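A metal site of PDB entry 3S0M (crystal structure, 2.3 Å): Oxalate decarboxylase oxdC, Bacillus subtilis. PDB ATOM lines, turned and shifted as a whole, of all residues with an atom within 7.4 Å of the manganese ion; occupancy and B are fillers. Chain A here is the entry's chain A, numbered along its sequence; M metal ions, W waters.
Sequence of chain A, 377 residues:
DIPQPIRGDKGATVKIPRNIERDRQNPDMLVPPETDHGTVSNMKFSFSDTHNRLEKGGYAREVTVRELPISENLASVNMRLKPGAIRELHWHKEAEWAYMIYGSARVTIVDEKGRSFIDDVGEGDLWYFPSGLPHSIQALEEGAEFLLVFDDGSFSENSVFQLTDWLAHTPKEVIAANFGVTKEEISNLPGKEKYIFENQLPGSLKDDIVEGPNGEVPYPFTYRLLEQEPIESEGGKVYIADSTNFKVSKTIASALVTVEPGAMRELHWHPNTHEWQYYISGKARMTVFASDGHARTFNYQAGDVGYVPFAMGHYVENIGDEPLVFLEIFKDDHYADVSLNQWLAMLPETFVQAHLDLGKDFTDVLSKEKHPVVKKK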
ATOM      1  N   ARG A 265      -3.662  -9.347 -28.853  1.00  0.00           N
ATOM      2  CA  ARG A 265      -3.115  -9.673 -27.562  1.00  0.00           C
ATOM      3  C   ARG A 265      -2.929 -11.183 -27.624  1.00  0.00           C
ATOM      4  O   ARG A 265      -3.873 -11.913 -27.935  1.00  0.00           O
ATOM      5  CB  ARG A 265      -4.119  -9.248 -26.478  1.00  0.00           C
ATOM      6  CG  ARG A 265      -3.751  -9.585 -25.057  1.00  0.00           C
ATOM      7  CD  ARG A 265      -2.660  -8.704 -24.475  1.00  0.00           C
ATOM      8  NE  ARG A 265      -2.313  -9.130 -23.111  1.00  0.00           N
ATOM      9  CZ  ARG A 265      -1.487 -10.139 -22.832  1.00  0.00           C
ATOM     10  NH1 ARG A 265      -0.891 -10.810 -23.820  1.00  0.00           N
ATOM     11  NH2 ARG A 265      -1.239 -10.471 -21.562  1.00  0.00           N
ATOM     12  N   GLU A 266      -1.698 -11.636 -27.388  1.00  0.00           N
ATOM     13  CA  GLU A 266      -1.305 -13.022 -27.686  1.00  0.00           C
ATOM     14  C   GLU A 266      -2.012 -14.048 -26.820  1.00  0.00           C
ATOM     15  O   GLU A 266      -2.761 -13.706 -25.897  1.00  0.00           O
ATOM     16  CB  GLU A 266       0.209 -13.207 -27.508  1.00  0.00           C
ATOM     17  CG  GLU A 266       0.662 -13.253 -26.050  1.00  0.00           C
ATOM     18  CD  GLU A 266       2.098 -13.696 -25.898  1.00  0.00           C
ATOM     19  OE1 GLU A 266       2.798 -13.187 -24.999  1.00  0.00           O
ATOM     20  OE2 GLU A 266       2.539 -14.546 -26.687  1.00  0.00           O
ATOM     21  N   HIS A 268      -2.484 -16.457 -23.943  1.00  0.00           N
ATOM     22  CA  HIS A 268      -1.959 -16.487 -22.574  1.00  0.00           C
ATOM     23  C   HIS A 268      -3.017 -16.877 -21.567  1.00  0.00           C
ATOM     24  O   HIS A 268      -4.177 -17.099 -21.930  1.00  0.00           O
ATOM     25  CB  HIS A 268      -1.413 -15.120 -22.176  1.00  0.00           C
ATOM     26  CG  HIS A 268      -2.460 -14.051 -22.093  1.00  0.00           C
ATOM     27  ND1 HIS A 268      -3.126 -13.579 -23.207  1.00  0.00           N
ATOM     28  CD2 HIS A 268      -2.946 -13.361 -21.029  1.00  0.00           C
ATOM     29  CE1 HIS A 268      -3.983 -12.644 -22.824  1.00  0.00           C
ATOM     30  NE2 HIS A 268      -3.891 -12.490 -21.515  1.00  0.00           N
ATOM     31  N   TRP A 269      -2.619 -16.983 -20.299  1.00  0.00           N
ATOM     32  CA  TRP A 269      -3.595 -16.989 -19.199  1.00  0.00           C
ATOM     33  C   TRP A 269      -3.026 -16.266 -18.007  1.00  0.00           C
ATOM     34  O   TRP A 269      -1.907 -15.748 -18.068  1.00  0.00           O
ATOM     35  CB  TRP A 269      -4.013 -18.384 -18.819  1.00  0.00           C
ATOM     36  CG  TRP A 269      -2.960 -19.234 -18.174  1.00  0.00           C
ATOM     37  CD1 TRP A 269      -2.714 -19.373 -16.827  1.00  0.00           C
ATOM     38  CD2 TRP A 269      -2.038 -20.113 -18.834  1.00  0.00           C
ATOM     39  NE1 TRP A 269      -1.693 -20.266 -16.631  1.00  0.00           N
ATOM     40  CE2 TRP A 269      -1.262 -20.734 -17.840  1.00  0.00           C
ATOM     41  CE3 TRP A 269      -1.792 -20.418 -20.180  1.00  0.00           C
ATOM     42  CZ2 TRP A 269      -0.252 -21.647 -18.144  1.00  0.00           C
ATOM     43  CZ3 TRP A 269      -0.782 -21.332 -20.485  1.00  0.00           C
ATOM     44  CH2 TRP A 269      -0.027 -21.939 -19.458  1.00  0.00           C
ATOM     45  N   HIS A 270      -3.788 -16.228 -16.923  1.00  0.00           N
ATOM     46  CA  HIS A 270      -3.301 -15.616 -15.693  1.00  0.00           C
ATOM     47  C   HIS A 270      -3.379 -16.604 -14.561  1.00  0.00           C
ATOM     48  O   HIS A 270      -4.440 -17.143 -14.268  1.00  0.00           O
ATOM     49  CB  HIS A 270      -4.114 -14.356 -15.375  1.00  0.00           C
ATOM     50  CG  HIS A 270      -4.139 -13.384 -16.501  1.00  0.00           C
ATOM     51  ND1 HIS A 270      -3.100 -12.508 -16.749  1.00  0.00           N
ATOM     52  CD2 HIS A 270      -5.050 -13.169 -17.479  1.00  0.00           C
ATOM     53  CE1 HIS A 270      -3.381 -11.792 -17.812  1.00  0.00           C
ATOM     54  NE2 HIS A 270      -4.551 -12.165 -18.279  1.00  0.00           N
ATOM     55  N   GLU A 275      -9.850 -12.340 -14.784  1.00  0.00           N
ATOM     56  CA  GLU A 275      -9.650 -11.102 -15.529  1.00  0.00           C
ATOM     57  C   GLU A 275     -10.969 -10.432 -15.824  1.00  0.00           C
ATOM     58  O   GLU A 275     -11.883 -11.039 -16.362  1.00  0.00           O
ATOM     59  CB  GLU A 275      -8.890 -11.317 -16.842  1.00  0.00           C
ATOM     60  CG  GLU A 275      -8.917 -10.064 -17.769  1.00  0.00           C
ATOM     61  CD  GLU A 275      -7.815 -10.061 -18.835  1.00  0.00           C
ATOM     62  OE1 GLU A 275      -8.070  -9.601 -19.972  1.00  0.00           O
ATOM     63  OE2 GLU A 275      -6.681 -10.488 -18.529  1.00  0.00           O
ATOM     64  N   GLN A 277     -12.653  -7.206 -17.852  1.00  0.00           N
ATOM     65  CA  GLN A 277     -12.260  -6.401 -19.002  1.00  0.00           C
ATOM     66  C   GLN A 277     -13.217  -5.266 -19.250  1.00  0.00           C
ATOM     67  O   GLN A 277     -14.435  -5.423 -19.125  1.00  0.00           O
ATOM     68  CB  GLN A 277     -12.229  -7.263 -20.261  1.00  0.00           C
ATOM     69  CG  GLN A 277     -11.248  -8.413 -20.267  1.00  0.00           C
ATOM     70  CD  GLN A 277     -11.320  -9.222 -21.566  1.00  0.00           C
ATOM     71  OE1 GLN A 277     -12.261  -9.090 -22.348  1.00  0.00           O
ATOM     72  NE2 GLN A 277     -10.309 -10.061 -21.790  1.00  0.00           N
ATOM     73  N   MET A 286     -12.662 -12.627 -28.552  1.00  0.00           N
ATOM     74  CA  MET A 286     -11.873 -13.417 -27.621  1.00  0.00           C
ATOM     75  C   MET A 286     -12.473 -14.810 -27.542  1.00  0.00           C
ATOM     76  O   MET A 286     -13.689 -14.964 -27.512  1.00  0.00           O
ATOM     77  CB  MET A 286     -11.855 -12.784 -26.228  1.00  0.00           C
ATOM     78  CG  MET A 286     -11.131 -13.619 -25.121  1.00  0.00           C
ATOM     79  SD  MET A 286     -11.219 -12.852 -23.457  1.00  0.00           S
ATOM     80  CE  MET A 286     -12.971 -12.539 -23.351  1.00  0.00           C
ATOM     81  N   VAL A 308     -12.621 -13.147 -17.949  1.00  0.00           N
ATOM     82  CA  VAL A 308     -11.981 -14.446 -18.108  1.00  0.00           C
ATOM     83  C   VAL A 308     -11.720 -15.092 -16.745  1.00  0.00           C
ATOM     84  O   VAL A 308     -10.844 -14.641 -15.988  1.00  0.00           O
ATOM     85  CB  VAL A 308     -10.618 -14.337 -18.816  1.00  0.00           C
ATOM     86  CG1 VAL A 308     -10.010 -15.724 -18.965  1.00  0.00           C
ATOM     87  CG2 VAL A 308     -10.747 -13.644 -20.167  1.00  0.00           C
ATOM     88  N   MET A 312      -8.191 -19.463 -17.324  1.00  0.00           N
ATOM     89  CA  MET A 312      -8.722 -19.829 -18.624  1.00  0.00           C
ATOM     90  C   MET A 312      -7.851 -19.230 -19.733  1.00  0.00           C
ATOM     91  O   MET A 312      -7.374 -18.096 -19.619  1.00  0.00           O
ATOM     92  CB  MET A 312     -10.186 -19.397 -18.780  1.00  0.00           C
ATOM     93  CG  MET A 312     -11.153 -20.165 -17.879  1.00  0.00           C
ATOM     94  SD  MET A 312     -12.882 -20.062 -18.422  1.00  0.00           S
ATOM     95  CE  MET A 312     -13.667 -21.135 -17.219  1.00  0.00           C
ATOM     96  N   HIS A 314      -6.886 -17.528 -23.192  1.00  0.00           N
ATOM     97  CA  HIS A 314      -7.532 -16.590 -24.088  1.00  0.00           C
ATOM     98  C   HIS A 314      -6.554 -15.814 -24.942  1.00  0.00           C
ATOM     99  O   HIS A 314      -5.335 -15.969 -24.826  1.00  0.00           O
ATOM    100  CB  HIS A 314      -8.378 -15.606 -23.278  1.00  0.00           C
ATOM    101  CG  HIS A 314      -7.637 -14.990 -22.147  1.00  0.00           C
ATOM    102  ND1 HIS A 314      -7.170 -15.714 -21.070  1.00  0.00           N
ATOM    103  CD2 HIS A 314      -7.286 -13.697 -21.911  1.00  0.00           C
ATOM    104  CE1 HIS A 314      -6.560 -14.902 -20.227  1.00  0.00           C
ATOM    105  NE2 HIS A 314      -6.624 -13.677 -20.706  1.00  0.00           N
ATOM    106  N   TYR A 315      -7.118 -14.981 -25.815  1.00  0.00           N
ATOM    107  CA  TYR A 315      -6.357 -14.076 -26.647  1.00  0.00           C
ATOM    108  C   TYR A 315      -7.344 -12.957 -26.945  1.00  0.00           C
ATOM    109  O   TYR A 315      -8.556 -13.143 -26.792  1.00  0.00           O
ATOM    110  CB  TYR A 315      -5.916 -14.754 -27.946  1.00  0.00           C
ATOM    111  CG  TYR A 315      -7.104 -15.154 -28.783  1.00  0.00           C
ATOM    112  CD1 TYR A 315      -7.635 -14.291 -29.740  1.00  0.00           C
ATOM    113  CD2 TYR A 315      -7.729 -16.369 -28.580  1.00  0.00           C
ATOM    114  CE1 TYR A 315      -8.748 -14.645 -30.479  1.00  0.00           C
ATOM    115  CE2 TYR A 315      -8.837 -16.732 -29.335  1.00  0.00           C
ATOM    116  CZ  TYR A 315      -9.343 -15.857 -30.266  1.00  0.00           C
ATOM    117  OH  TYR A 315     -10.461 -16.235 -30.983  1.00  0.00           O
ATOM    118  N   VAL A 316      -6.848 -11.795 -27.368  1.00  0.00           N
ATOM    119  CA  VAL A 316      -7.750 -10.733 -27.782  1.00  0.00           C
ATOM    120  C   VAL A 316      -7.343 -10.229 -29.152  1.00  0.00           C
ATOM    121  O   VAL A 316      -6.300  -9.589 -29.313  1.00  0.00           O
ATOM    122  CB  VAL A 316      -7.787  -9.595 -26.760  1.00  0.00           C
ATOM    123  CG1 VAL A 316      -8.898  -8.637 -27.103  1.00  0.00           C
ATOM    124  CG2 VAL A 316      -7.996 -10.173 -25.353  1.00  0.00           C
ATOM    125  N   PHE A 326      -8.332  -1.560 -24.624  1.00  0.00           N
ATOM    126  CA  PHE A 326      -9.110  -2.114 -23.528  1.00  0.00           C
ATOM    127  C   PHE A 326      -8.309  -2.227 -22.253  1.00  0.00           C
ATOM    128  O   PHE A 326      -7.091  -2.142 -22.259  1.00  0.00           O
ATOM    129  CB  PHE A 326      -9.734  -3.457 -23.908  1.00  0.00           C
ATOM    130  CG  PHE A 326      -8.750  -4.580 -24.068  1.00  0.00           C
ATOM    131  CD1 PHE A 326      -8.491  -5.450 -23.028  1.00  0.00           C
ATOM    132  CD2 PHE A 326      -8.105  -4.793 -25.282  1.00  0.00           C
ATOM    133  CE1 PHE A 326      -7.601  -6.503 -23.186  1.00  0.00           C
ATOM    134  CE2 PHE A 326      -7.211  -5.851 -25.449  1.00  0.00           C
ATOM    135  CZ  PHE A 326      -6.952  -6.700 -24.396  1.00  0.00           C
ATOM    136  N   GLU A 328      -7.391  -4.427 -18.712  1.00  0.00           N
ATOM    137  CA  GLU A 328      -7.381  -5.713 -18.010  1.00  0.00           C
ATOM    138  C   GLU A 328      -7.311  -5.471 -16.507  1.00  0.00           C
ATOM    139  O   GLU A 328      -6.340  -4.879 -16.022  1.00  0.00           O
ATOM    140  CB  GLU A 328      -6.159  -6.544 -18.422  1.00  0.00           C
ATOM    141  CG  GLU A 328      -6.213  -7.109 -19.826  1.00  0.00           C
ATOM    142  CD  GLU A 328      -4.844  -7.505 -20.334  1.00  0.00           C
ATOM    143  OE1 GLU A 328      -3.845  -7.131 -19.683  1.00  0.00           O
ATOM    144  OE2 GLU A 328      -4.771  -8.176 -21.381  1.00  0.00           O
ATOM    145  N   PHE A 330      -7.526  -7.048 -12.464  1.00  0.00           N
ATOM    146  CA  PHE A 330      -7.463  -8.209 -11.583  1.00  0.00           C
ATOM    147  C   PHE A 330      -7.636  -7.808 -10.117  1.00  0.00           C
ATOM    148  O   PHE A 330      -7.250  -6.699  -9.705  1.00  0.00           O
ATOM    149  CB  PHE A 330      -6.146  -8.952 -11.781  1.00  0.00           C
ATOM    150  CG  PHE A 330      -5.829  -9.212 -13.207  1.00  0.00           C
ATOM    151  CD1 PHE A 330      -6.087 -10.447 -13.768  1.00  0.00           C
ATOM    152  CD2 PHE A 330      -5.295  -8.218 -14.001  1.00  0.00           C
ATOM    153  CE1 PHE A 330      -5.811 -10.697 -15.097  1.00  0.00           C
ATOM    154  CE2 PHE A 330      -5.027  -8.447 -15.331  1.00  0.00           C
ATOM    155  CZ  PHE A 330      -5.280  -9.699 -15.883  1.00  0.00           C
ATOM    156  N   TYR A 335       0.138  -7.936 -11.357  1.00  0.00           N
ATOM    157  CA  TYR A 335      -0.210  -8.458 -12.666  1.00  0.00           C
ATOM    158  C   TYR A 335       0.703  -9.624 -12.959  1.00  0.00           C
ATOM    159  O   TYR A 335       1.861  -9.626 -12.566  1.00  0.00           O
ATOM    160  CB  TYR A 335       0.000  -7.410 -13.745  1.00  0.00           C
ATOM    161  CG  TYR A 335      -0.358  -7.871 -15.147  1.00  0.00           C
ATOM    162  CD1 TYR A 335      -1.593  -7.559 -15.690  1.00  0.00           C
ATOM    163  CD2 TYR A 335       0.557  -8.579 -15.919  1.00  0.00           C
ATOM    164  CE1 TYR A 335      -1.918  -7.959 -16.969  1.00  0.00           C
ATOM    165  CE2 TYR A 335       0.232  -8.980 -17.199  1.00  0.00           C
ATOM    166  CZ  TYR A 335      -1.004  -8.676 -17.714  1.00  0.00           C
ATOM    167  OH  TYR A 335      -1.344  -9.067 -18.992  1.00  0.00           O
ATOM    168  N   ALA A 336       0.187 -10.611 -13.680  1.00  0.00           N
ATOM    169  CA  ALA A 336       0.994 -11.760 -14.032  1.00  0.00           C
ATOM    170  C   ALA A 336       0.286 -12.496 -15.138  1.00  0.00           C
ATOM    171  O   ALA A 336      -0.946 -12.523 -15.190  1.00  0.00           O
ATOM    172  CB  ALA A 336       1.216 -12.684 -12.825  1.00  0.00           C
ATOM    173  N   ASP A 337       1.072 -13.076 -16.033  1.00  0.00           N
ATOM    174  CA  ASP A 337       0.533 -13.902 -17.091  1.00  0.00           C
ATOM    175  C   ASP A 337       1.547 -14.935 -17.534  1.00  0.00           C
ATOM    176  O   ASP A 337       2.747 -14.786 -17.308  1.00  0.00           O
ATOM    177  CB  ASP A 337       0.109 -13.046 -18.290  1.00  0.00           C
ATOM    178  CG  ASP A 337       1.300 -12.418 -19.016  1.00  0.00           C
ATOM    179  OD1 ASP A 337       2.387 -12.326 -18.413  1.00  0.00           O
ATOM    180  OD2 ASP A 337       1.147 -12.008 -20.185  1.00  0.00           O
HETATM  181 MN    MN M   1      -5.655 -11.667 -20.199  1.00  0.00          MN
HETATM  182  O   HOH W   1      -6.316 -10.286 -21.985  1.00  0.00           O
HETATM  183  O   HOH W   2      -4.104 -10.178 -19.997  1.00  0.00           O
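ND1 of His 270 lies within hydrogen-bond range of O of Ala 336. The side-chain carboxylate (OE1) of Glu 275 is in hydrogen-bond range of the side-chain amide nitrogen (NE2) of Gln 277, at 2.9 Å. The backbone carbonyl oxygen (O) of Glu 275 sits at hydrogen-bond distance from the backbone NH (N) of Val 308. The backbone carbonyl oxygen (O) of Met 312 sits at hydrogen-bond distance from a ring nitrogen (ND1) of His 314. NE2 of His 268 lies close to NH2 of Arg 265, at 3.3 Å. A ring nitrogen (ND1) of His 268 sits at hydrogen-bond distance from the backbone carbonyl oxygen (O) of Glu 266 (2.7 Å). OE2 of Glu 328 is in salt-bridge range of NE of Arg 265, at 3.2 Å. The side-chain carboxylate (OE1) of Glu 328 lies within hydrogen-bond range of the side-chain hydroxyl (OH) of Tyr 335.
Merely in contact with the manganese ion: Glu 328 (3.8 Å). Of the 19 residues printed, 5 come within 4 Å of the manganese ion. Along chain A the residues within 4 Å of the manganese ion span positions 268 to 328.
Water W2 binds the manganese ion, 2.2 Å away. The manganese ion is bound by a ring nitrogen (NE2) of His 270 (2.3 Å). OE2 of Glu 275 is bound to the manganese ion (2.3 Å). The manganese ion is bound by a ring nitrogen (NE2) of His 314 (2.3 Å). The manganese ion is bound by NE2 of His 268 (2.3 Å). Water W1 is bound to the manganese ion (2.4 Å).
Water W1 lies within hydrogen-bond range of OE2 of Glu 328 (2.7 Å) and OE1 of Glu 275 (2.8 Å). Water W2 lies within hydrogen-bond range of OE2 of Glu 328 (2.5 Å), OH of Tyr 335 (3.1 Å) and NH2 of Arg 265 (3.3 Å).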
